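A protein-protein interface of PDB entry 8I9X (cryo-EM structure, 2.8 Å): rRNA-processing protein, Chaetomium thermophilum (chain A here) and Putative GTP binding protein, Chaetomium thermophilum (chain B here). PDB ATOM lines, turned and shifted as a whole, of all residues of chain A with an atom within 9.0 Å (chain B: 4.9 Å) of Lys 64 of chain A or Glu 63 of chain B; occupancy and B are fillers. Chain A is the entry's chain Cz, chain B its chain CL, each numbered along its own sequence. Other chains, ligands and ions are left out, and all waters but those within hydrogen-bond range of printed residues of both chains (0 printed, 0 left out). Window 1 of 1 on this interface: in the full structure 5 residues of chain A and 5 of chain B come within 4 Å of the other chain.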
ATOM      1  N   LYS A  54      27.456  17.818   7.022  1.00  0.00           N
ATOM      2  CA  LYS A  54      26.268  17.200   6.443  1.00  0.00           C
ATOM      3  C   LYS A  54      26.615  16.317   5.252  1.00  0.00           C
ATOM      4  O   LYS A  54      25.983  15.277   5.047  1.00  0.00           O
ATOM      5  CB  LYS A  54      25.250  18.270   6.049  1.00  0.00           C
ATOM      6  CG  LYS A  54      24.739  19.132   7.201  1.00  0.00           C
ATOM      7  CD  LYS A  54      23.815  18.352   8.143  1.00  0.00           C
ATOM      8  CE  LYS A  54      24.545  17.745   9.333  1.00  0.00           C
ATOM      9  NZ  LYS A  54      23.609  17.086  10.285  1.00  0.00           N
ATOM     10  N   GLU A  57      27.908  13.044   6.720  1.00  0.00           N
ATOM     11  CA  GLU A  57      26.769  12.269   7.190  1.00  0.00           C
ATOM     12  C   GLU A  57      25.947  11.673   6.055  1.00  0.00           C
ATOM     13  O   GLU A  57      25.519  10.519   6.159  1.00  0.00           O
ATOM     14  CB  GLU A  57      25.863  13.134   8.070  1.00  0.00           C
ATOM     15  CG  GLU A  57      24.977  12.332   9.003  1.00  0.00           C
ATOM     16  CD  GLU A  57      23.687  13.051   9.338  1.00  0.00           C
ATOM     17  OE1 GLU A  57      23.592  14.265   9.056  1.00  0.00           O
ATOM     18  OE2 GLU A  57      22.767  12.403   9.876  1.00  0.00           O
ATOM     19  N   GLN A  58      25.717  12.429   4.979  1.00  0.00           N
ATOM     20  CA  GLN A  58      24.997  11.898   3.824  1.00  0.00           C
ATOM     21  C   GLN A  58      25.789  10.791   3.137  1.00  0.00           C
ATOM     22  O   GLN A  58      25.207   9.829   2.621  1.00  0.00           O
ATOM     23  CB  GLN A  58      24.685  13.027   2.842  1.00  0.00           C
ATOM     24  CG  GLN A  58      24.015  12.572   1.556  1.00  0.00           C
ATOM     25  CD  GLN A  58      22.614  12.044   1.788  1.00  0.00           C
ATOM     26  OE1 GLN A  58      22.399  10.834   1.866  1.00  0.00           O
ATOM     27  NE2 GLN A  58      21.651  12.951   1.902  1.00  0.00           N
ATOM     28  N   ALA A  59      27.116  10.921   3.096  1.00  0.00           N
ATOM     29  CA  ALA A  59      27.941   9.855   2.544  1.00  0.00           C
ATOM     30  C   ALA A  59      27.791   8.569   3.345  1.00  0.00           C
ATOM     31  O   ALA A  59      27.654   7.488   2.758  1.00  0.00           O
ATOM     32  CB  ALA A  59      29.407  10.288   2.502  1.00  0.00           C
ATOM     33  N   ALA A  60      27.800   8.667   4.678  1.00  0.00           N
ATOM     34  CA  ALA A  60      27.533   7.483   5.495  1.00  0.00           C
ATOM     35  C   ALA A  60      26.126   6.940   5.256  1.00  0.00           C
ATOM     36  O   ALA A  60      25.935   5.715   5.170  1.00  0.00           O
ATOM     37  CB  ALA A  60      27.731   7.805   6.975  1.00  0.00           C
ATOM     38  N   MET A  61      25.140   7.840   5.164  1.00  0.00           N
ATOM     39  CA  MET A  61      23.773   7.468   4.807  1.00  0.00           C
ATOM     40  C   MET A  61      23.751   6.574   3.578  1.00  0.00           C
ATOM     41  O   MET A  61      23.262   5.438   3.630  1.00  0.00           O
ATOM     42  CB  MET A  61      22.953   8.727   4.510  1.00  0.00           C
ATOM     43  CG  MET A  61      21.447   8.641   4.734  1.00  0.00           C
ATOM     44  SD  MET A  61      20.913   7.638   6.121  1.00  0.00           S
ATOM     45  CE  MET A  61      21.771   8.513   7.431  1.00  0.00           C
ATOM     46  N   LYS A  62      24.281   7.081   2.466  1.00  0.00           N
ATOM     47  CA  LYS A  62      24.296   6.374   1.196  1.00  0.00           C
ATOM     48  C   LYS A  62      25.093   5.081   1.253  1.00  0.00           C
ATOM     49  O   LYS A  62      24.662   4.087   0.661  1.00  0.00           O
ATOM     50  CB  LYS A  62      24.855   7.286   0.100  1.00  0.00           C
ATOM     51  CG  LYS A  62      23.950   8.461  -0.247  1.00  0.00           C
ATOM     52  CD  LYS A  62      24.526   9.295  -1.381  1.00  0.00           C
ATOM     53  CE  LYS A  62      23.539  10.357  -1.840  1.00  0.00           C
ATOM     54  NZ  LYS A  62      24.001  11.050  -3.074  1.00  0.00           N
ATOM     55  N   ALA A  63      26.232   5.067   1.950  1.00  0.00           N
ATOM     56  CA  ALA A  63      27.010   3.838   2.053  1.00  0.00           C
ATOM     57  C   ALA A  63      26.216   2.734   2.739  1.00  0.00           C
ATOM     58  O   ALA A  63      26.132   1.609   2.223  1.00  0.00           O
ATOM     59  CB  ALA A  63      28.317   4.104   2.799  1.00  0.00           C
ATOM     60  N   LYS A  64      25.604   3.031   3.889  1.00  0.00           N
ATOM     61  CA  LYS A  64      24.877   1.970   4.574  1.00  0.00           C
ATOM     62  C   LYS A  64      23.586   1.595   3.852  1.00  0.00           C
ATOM     63  O   LYS A  64      23.200   0.419   3.873  1.00  0.00           O
ATOM     64  CB  LYS A  64      24.585   2.350   6.029  1.00  0.00           C
ATOM     65  CG  LYS A  64      23.370   3.212   6.259  1.00  0.00           C
ATOM     66  CD  LYS A  64      23.150   3.385   7.751  1.00  0.00           C
ATOM     67  CE  LYS A  64      21.806   4.017   8.046  1.00  0.00           C
ATOM     68  NZ  LYS A  64      21.753   5.410   7.575  1.00  0.00           N
ATOM     69  N   GLU A  65      22.929   2.553   3.188  1.00  0.00           N
ATOM     70  CA  GLU A  65      21.756   2.222   2.383  1.00  0.00           C
ATOM     71  C   GLU A  65      22.122   1.297   1.228  1.00  0.00           C
ATOM     72  O   GLU A  65      21.402   0.331   0.945  1.00  0.00           O
ATOM     73  CB  GLU A  65      21.103   3.504   1.863  1.00  0.00           C
ATOM     74  CG  GLU A  65      19.782   3.280   1.150  1.00  0.00           C
ATOM     75  CD  GLU A  65      19.066   4.575   0.813  1.00  0.00           C
ATOM     76  OE1 GLU A  65      19.610   5.656   1.119  1.00  0.00           O
ATOM     77  OE2 GLU A  65      17.958   4.512   0.241  1.00  0.00           O
ATOM     78  N   ARG A  66      23.237   1.578   0.546  1.00  0.00           N
ATOM     79  CA  ARG A  66      23.686   0.701  -0.527  1.00  0.00           C
ATOM     80  C   ARG A  66      24.042  -0.682  -0.006  1.00  0.00           C
ATOM     81  O   ARG A  66      23.727  -1.683  -0.660  1.00  0.00           O
ATOM     82  CB  ARG A  66      24.884   1.317  -1.252  1.00  0.00           C
ATOM     83  CG  ARG A  66      24.517   2.354  -2.303  1.00  0.00           C
ATOM     84  CD  ARG A  66      25.759   2.941  -2.956  1.00  0.00           C
ATOM     85  NE  ARG A  66      25.427   3.954  -3.951  1.00  0.00           N
ATOM     86  CZ  ARG A  66      26.324   4.657  -4.631  1.00  0.00           C
ATOM     87  NH1 ARG A  66      27.622   4.481  -4.450  1.00  0.00           N
ATOM     88  NH2 ARG A  66      25.905   5.559  -5.515  1.00  0.00           N
ATOM     89  N   GLU A  67      24.696  -0.761   1.156  1.00  0.00           N
ATOM     90  CA  GLU A  67      25.006  -2.070   1.725  1.00  0.00           C
ATOM     91  C   GLU A  67      23.734  -2.853   2.033  1.00  0.00           C
ATOM     92  O   GLU A  67      23.647  -4.055   1.740  1.00  0.00           O
ATOM     93  CB  GLU A  67      25.855  -1.908   2.985  1.00  0.00           C
ATOM     94  CG  GLU A  67      26.496  -3.198   3.469  1.00  0.00           C
ATOM     95  CD  GLU A  67      25.700  -3.865   4.573  1.00  0.00           C
ATOM     96  OE1 GLU A  67      24.960  -3.156   5.287  1.00  0.00           O
ATOM     97  OE2 GLU A  67      25.814  -5.098   4.726  1.00  0.00           O
ATOM     98  N   MET A  68      22.734  -2.185   2.616  1.00  0.00           N
ATOM     99  CA  MET A  68      21.468  -2.845   2.914  1.00  0.00           C
ATOM    100  C   MET A  68      20.788  -3.341   1.644  1.00  0.00           C
ATOM    101  O   MET A  68      20.314  -4.484   1.590  1.00  0.00           O
ATOM    102  CB  MET A  68      20.546  -1.885   3.663  1.00  0.00           C
ATOM    103  CG  MET A  68      20.630  -1.975   5.172  1.00  0.00           C
ATOM    104  SD  MET A  68      19.301  -1.049   5.958  1.00  0.00           S
ATOM    105  CE  MET A  68      20.156  -0.382   7.378  1.00  0.00           C
ATOM    106  N   LYS A  69      20.728  -2.495   0.612  1.00  0.00           N
ATOM    107  CA  LYS A  69      20.095  -2.907  -0.635  1.00  0.00           C
ATOM    108  C   LYS A  69      20.836  -4.068  -1.282  1.00  0.00           C
ATOM    109  O   LYS A  69      20.200  -5.002  -1.786  1.00  0.00           O
ATOM    110  CB  LYS A  69      20.004  -1.728  -1.604  1.00  0.00           C
ATOM    111  CG  LYS A  69      19.146  -0.560  -1.120  1.00  0.00           C
ATOM    112  CD  LYS A  69      17.654  -0.883  -1.153  1.00  0.00           C
ATOM    113  CE  LYS A  69      17.123  -1.278   0.220  1.00  0.00           C
ATOM    114  NZ  LYS A  69      15.649  -1.485   0.213  1.00  0.00           N
ATOM    115  N   GLU A  70      22.172  -4.036  -1.272  1.00  0.00           N
ATOM    116  CA  GLU A  70      22.942  -5.120  -1.871  1.00  0.00           C
ATOM    117  C   GLU A  70      22.714  -6.436  -1.139  1.00  0.00           C
ATOM    118  O   GLU A  70      22.519  -7.479  -1.777  1.00  0.00           O
ATOM    119  CB  GLU A  70      24.428  -4.763  -1.887  1.00  0.00           C
ATOM    120  CG  GLU A  70      24.847  -3.923  -3.082  1.00  0.00           C
ATOM    121  CD  GLU A  70      26.306  -3.518  -3.028  1.00  0.00           C
ATOM    122  OE1 GLU A  70      26.921  -3.645  -1.948  1.00  0.00           O
ATOM    123  OE2 GLU A  70      26.840  -3.074  -4.066  1.00  0.00           O
ATOM    124  N   GLU A  71      22.727  -6.414   0.198  1.00  0.00           N
ATOM    125  CA  GLU A  71      22.507  -7.661   0.926  1.00  0.00           C
ATOM    126  C   GLU A  71      21.084  -8.182   0.747  1.00  0.00           C
ATOM    127  O   GLU A  71      20.887  -9.398   0.613  1.00  0.00           O
ATOM    128  CB  GLU A  71      22.849  -7.486   2.411  1.00  0.00           C
ATOM    129  CG  GLU A  71      21.958  -6.537   3.193  1.00  0.00           C
ATOM    130  CD  GLU A  71      20.771  -7.237   3.826  1.00  0.00           C
ATOM    131  OE1 GLU A  71      20.834  -8.472   4.004  1.00  0.00           O
ATOM    132  OE2 GLU A  71      19.775  -6.554   4.146  1.00  0.00           O
ATOM    133  N   LYS A  72      20.086  -7.291   0.716  1.00  0.00           N
ATOM    134  CA  LYS A  72      18.717  -7.736   0.477  1.00  0.00           C
ATOM    135  C   LYS A  72      18.566  -8.336  -0.917  1.00  0.00           C
ATOM    136  O   LYS A  72      17.893  -9.362  -1.089  1.00  0.00           O
ATOM    137  CB  LYS A  72      17.744  -6.575   0.672  1.00  0.00           C
ATOM    138  CG  LYS A  72      16.403  -6.985   1.261  1.00  0.00           C
ATOM    139  CD  LYS A  72      15.558  -5.773   1.620  1.00  0.00           C
ATOM    140  CE  LYS A  72      14.366  -6.167   2.478  1.00  0.00           C
ATOM    141  NZ  LYS A  72      13.581  -7.276   1.867  1.00  0.00           N
ATOM    142  N   PRO B  60      16.315  13.995   9.170  1.00  0.00           N
ATOM    143  CA  PRO B  60      17.612  14.063   9.863  1.00  0.00           C
ATOM    144  C   PRO B  60      17.898  12.889  10.784  1.00  0.00           C
ATOM    145  O   PRO B  60      19.033  12.767  11.259  1.00  0.00           O
ATOM    146  CB  PRO B  60      17.512  15.377  10.645  1.00  0.00           C
ATOM    147  CG  PRO B  60      16.049  15.521  10.904  1.00  0.00           C
ATOM    148  CD  PRO B  60      15.391  15.039   9.641  1.00  0.00           C
ATOM    149  N   TYR B  61      16.924  12.026  11.055  1.00  0.00           N
ATOM    150  CA  TYR B  61      17.100  10.912  11.983  1.00  0.00           C
ATOM    151  C   TYR B  61      16.910   9.586  11.263  1.00  0.00           C
ATOM    152  O   TYR B  61      16.541   8.563  11.851  1.00  0.00           O
ATOM    153  CB  TYR B  61      16.154  11.057  13.168  1.00  0.00           C
ATOM    154  CG  TYR B  61      16.234  12.422  13.808  1.00  0.00           C
ATOM    155  CD1 TYR B  61      17.462  12.987  14.115  1.00  0.00           C
ATOM    156  CD2 TYR B  61      15.088  13.145  14.105  1.00  0.00           C
ATOM    157  CE1 TYR B  61      17.550  14.228  14.698  1.00  0.00           C
ATOM    158  CE2 TYR B  61      15.167  14.392  14.691  1.00  0.00           C
ATOM    159  CZ  TYR B  61      16.402  14.927  14.984  1.00  0.00           C
ATOM    160  OH  TYR B  61      16.497  16.167  15.565  1.00  0.00           O
ATOM    161  N   LYS B  62      17.182   9.597   9.958  1.00  0.00           N
ATOM    162  CA  LYS B  62      17.089   8.381   9.161  1.00  0.00           C
ATOM    163  C   LYS B  62      18.083   7.328   9.637  1.00  0.00           C
ATOM    164  O   LYS B  62      17.747   6.140   9.693  1.00  0.00           O
ATOM    165  CB  LYS B  62      17.306   8.711   7.684  1.00  0.00           C
ATOM    166  CG  LYS B  62      17.095   7.541   6.741  1.00  0.00           C
ATOM    167  CD  LYS B  62      17.211   7.981   5.292  1.00  0.00           C
ATOM    168  CE  LYS B  62      17.339   6.790   4.358  1.00  0.00           C
ATOM    169  NZ  LYS B  62      17.142   7.182   2.935  1.00  0.00           N
ATOM    170  N   GLU B  63      19.302   7.743   9.994  1.00  0.00           N
ATOM    171  CA  GLU B  63      20.292   6.785  10.479  1.00  0.00           C
ATOM    172  C   GLU B  63      19.815   6.102  11.754  1.00  0.00           C
ATOM    173  O   GLU B  63      19.945   4.881  11.902  1.00  0.00           O
ATOM    174  CB  GLU B  63      21.642   7.475  10.702  1.00  0.00           C
ATOM    175  CG  GLU B  63      21.706   8.473  11.855  1.00  0.00           C
ATOM    176  CD  GLU B  63      21.228   9.859  11.463  1.00  0.00           C
ATOM    177  OE1 GLU B  63      20.574   9.993  10.407  1.00  0.00           O
ATOM    178  OE2 GLU B  63      21.515  10.817  12.212  1.00  0.00           O
ATOM    179  N   ARG B  64      19.238   6.869  12.681  1.00  0.00           N
ATOM    180  CA  ARG B  64      18.779   6.272  13.927  1.00  0.00           C
ATOM    181  C   ARG B  64      17.578   5.373  13.690  1.00  0.00           C
ATOM    182  O   ARG B  64      17.445   4.322  14.327  1.00  0.00           O
ATOM    183  CB  ARG B  64      18.450   7.353  14.957  1.00  0.00           C
ATOM    184  CG  ARG B  64      19.646   8.188  15.381  1.00  0.00           C
ATOM    185  CD  ARG B  64      19.314   9.062  16.579  1.00  0.00           C
ATOM    186  NE  ARG B  64      18.281  10.054  16.309  1.00  0.00           N
ATOM    187  CZ  ARG B  64      17.703  10.795  17.243  1.00  0.00           C
ATOM    188  NH1 ARG B  64      18.036  10.680  18.519  1.00  0.00           N
ATOM    189  NH2 ARG B  64      16.765  11.669  16.893  1.00  0.00           N
ATOM    190  N   LEU B  65      16.690   5.762  12.772  1.00  0.00           N
ATOM    191  CA  LEU B  65      15.545   4.903  12.496  1.00  0.00           C
ATOM    192  C   LEU B  65      15.991   3.583  11.876  1.00  0.00           C
ATOM    193  O   LEU B  65      15.490   2.519  12.257  1.00  0.00           O
ATOM    194  CB  LEU B  65      14.544   5.623  11.591  1.00  0.00           C
ATOM    195  CG  LEU B  65      13.134   5.026  11.492  1.00  0.00           C
ATOM    196  CD1 LEU B  65      12.127   6.123  11.172  1.00  0.00           C
ATOM    197  CD2 LEU B  65      13.027   3.897  10.482  1.00  0.00           C
ATOM    198  N   LEU B  66      16.939   3.627  10.935  1.00  0.00           N
ATOM    199  CA  LEU B  66      17.463   2.392  10.356  1.00  0.00           C
ATOM    200  C   LEU B  66      18.176   1.541  11.401  1.00  0.00           C
ATOM    201  O   LEU B  66      18.065   0.308  11.385  1.00  0.00           O
ATOM    202  CB  LEU B  66      18.400   2.694   9.184  1.00  0.00           C
ATOM    203  CG  LEU B  66      17.810   2.892   7.782  1.00  0.00           C
ATOM    204  CD1 LEU B  66      17.156   1.606   7.300  1.00  0.00           C
ATOM    205  CD2 LEU B  66      16.819   4.030   7.715  1.00  0.00           C
ATOM    206  N   GLN B  67      18.928   2.172  12.306  1.00  0.00           N
ATOM    207  CA  GLN B  67      19.579   1.411  13.367  1.00  0.00           C
ATOM    208  C   GLN B  67      18.556   0.727  14.266  1.00  0.00           C
ATOM    209  O   GLN B  67      18.743  -0.439  14.645  1.00  0.00           O
ATOM    210  CB  GLN B  67      20.493   2.327  14.183  1.00  0.00           C
ATOM    211  CG  GLN B  67      21.373   1.606  15.196  1.00  0.00           C
ATOM    212  CD  GLN B  67      20.680   1.370  16.524  1.00  0.00           C
ATOM    213  OE1 GLN B  67      19.809   2.141  16.927  1.00  0.00           O
ATOM    214  NE2 GLN B  67      21.064   0.301  17.210  1.00  0.00           N
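OE2 of Glu 63 of chain B sits close to OE2 of Glu 57 of chain A (3.1 Å). NZ of Lys 62 of chain B is in salt-bridge range of OE1 of Glu 65 of chain A (3.4 Å).
OE2 of Glu 57 of chain A touches O of Pro 60 of chain B, at 3.998 Å. CD of Lys 62 of chain B touches SD of Met 61 of chain A, 3.8 Å away. Glu 63 of chain B touches Met 61 of chain A (CB to CE, 3.4 Å). NZ of Lys 64 of chain A touches CA of Glu 63 of chain B, 3.5 Å away. Leu 66 of chain B touches Lys 64 of chain A (CB to CE, 3.8 Å). Leu 66 of chain B touches Met 68 of chain A.
The side-chain sulfur (SD) of Met 61 of chain A sits at hydrogen-bond distance from the side-chain amino group (NZ) of Lys 64 of chain A, 2.8 Å away. The side-chain amino group (NZ) of Lys 54 of chain A is in salt-bridge range of the side-chain carboxylate (OE1) of Glu 57 of chain A, at 3.1 Å.
Of the 8 printed residues of chain B, 4 touch a printed residue of chain A. Of the 17 printed residues of chain A, 5 touch a printed residue of chain B. Printed residues of chain A that touch a printed residue of chain B: Glu 57, Met 61, Lys 64, Glu 65 and Met 68. Hydrophobic or aromatic side chains of chain A that line the printed part of chain B: Met 61 and Met 68. Along chain A the printed residues that touch a printed residue of chain B span positions 57 to 68. Among the printed residues, 8 pairs touch across the chains. Among the printed residues, Asp or Glu carboxylates within 4 Å of a Lys or Arg side-chain nitrogen of the other chain: Glu 65 of chain A with Lys 62 of chain B (3.4 Å).
Of chain B, only Glu 63 (3.5 Å) and Leu 66 (3.8 Å) come within 4 Å of Lys 64 of chain A. Glu 63 of chain B touches just these residues of chain A: Glu 57, Met 61 and Lys 64. Of the printed residues of chain B, Glu 65 of chain A touches Lys 62. Of the printed residues of chain A, Leu 66 of chain B touches Lys 64 (3.8 Å) and Met 68 (3.6 Å). Of the printed residues of chain B, Met 61 of chain A touches Lys 62 and Glu 63. The nearest residue of chain B that does not touch Lys 64 of chain A is Lys 62 of chain B (4.6 Å). The nearest printed residue of chain A that does not touch Lys 62 of chain B is Lys 64 of chain A (4.6 Å).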
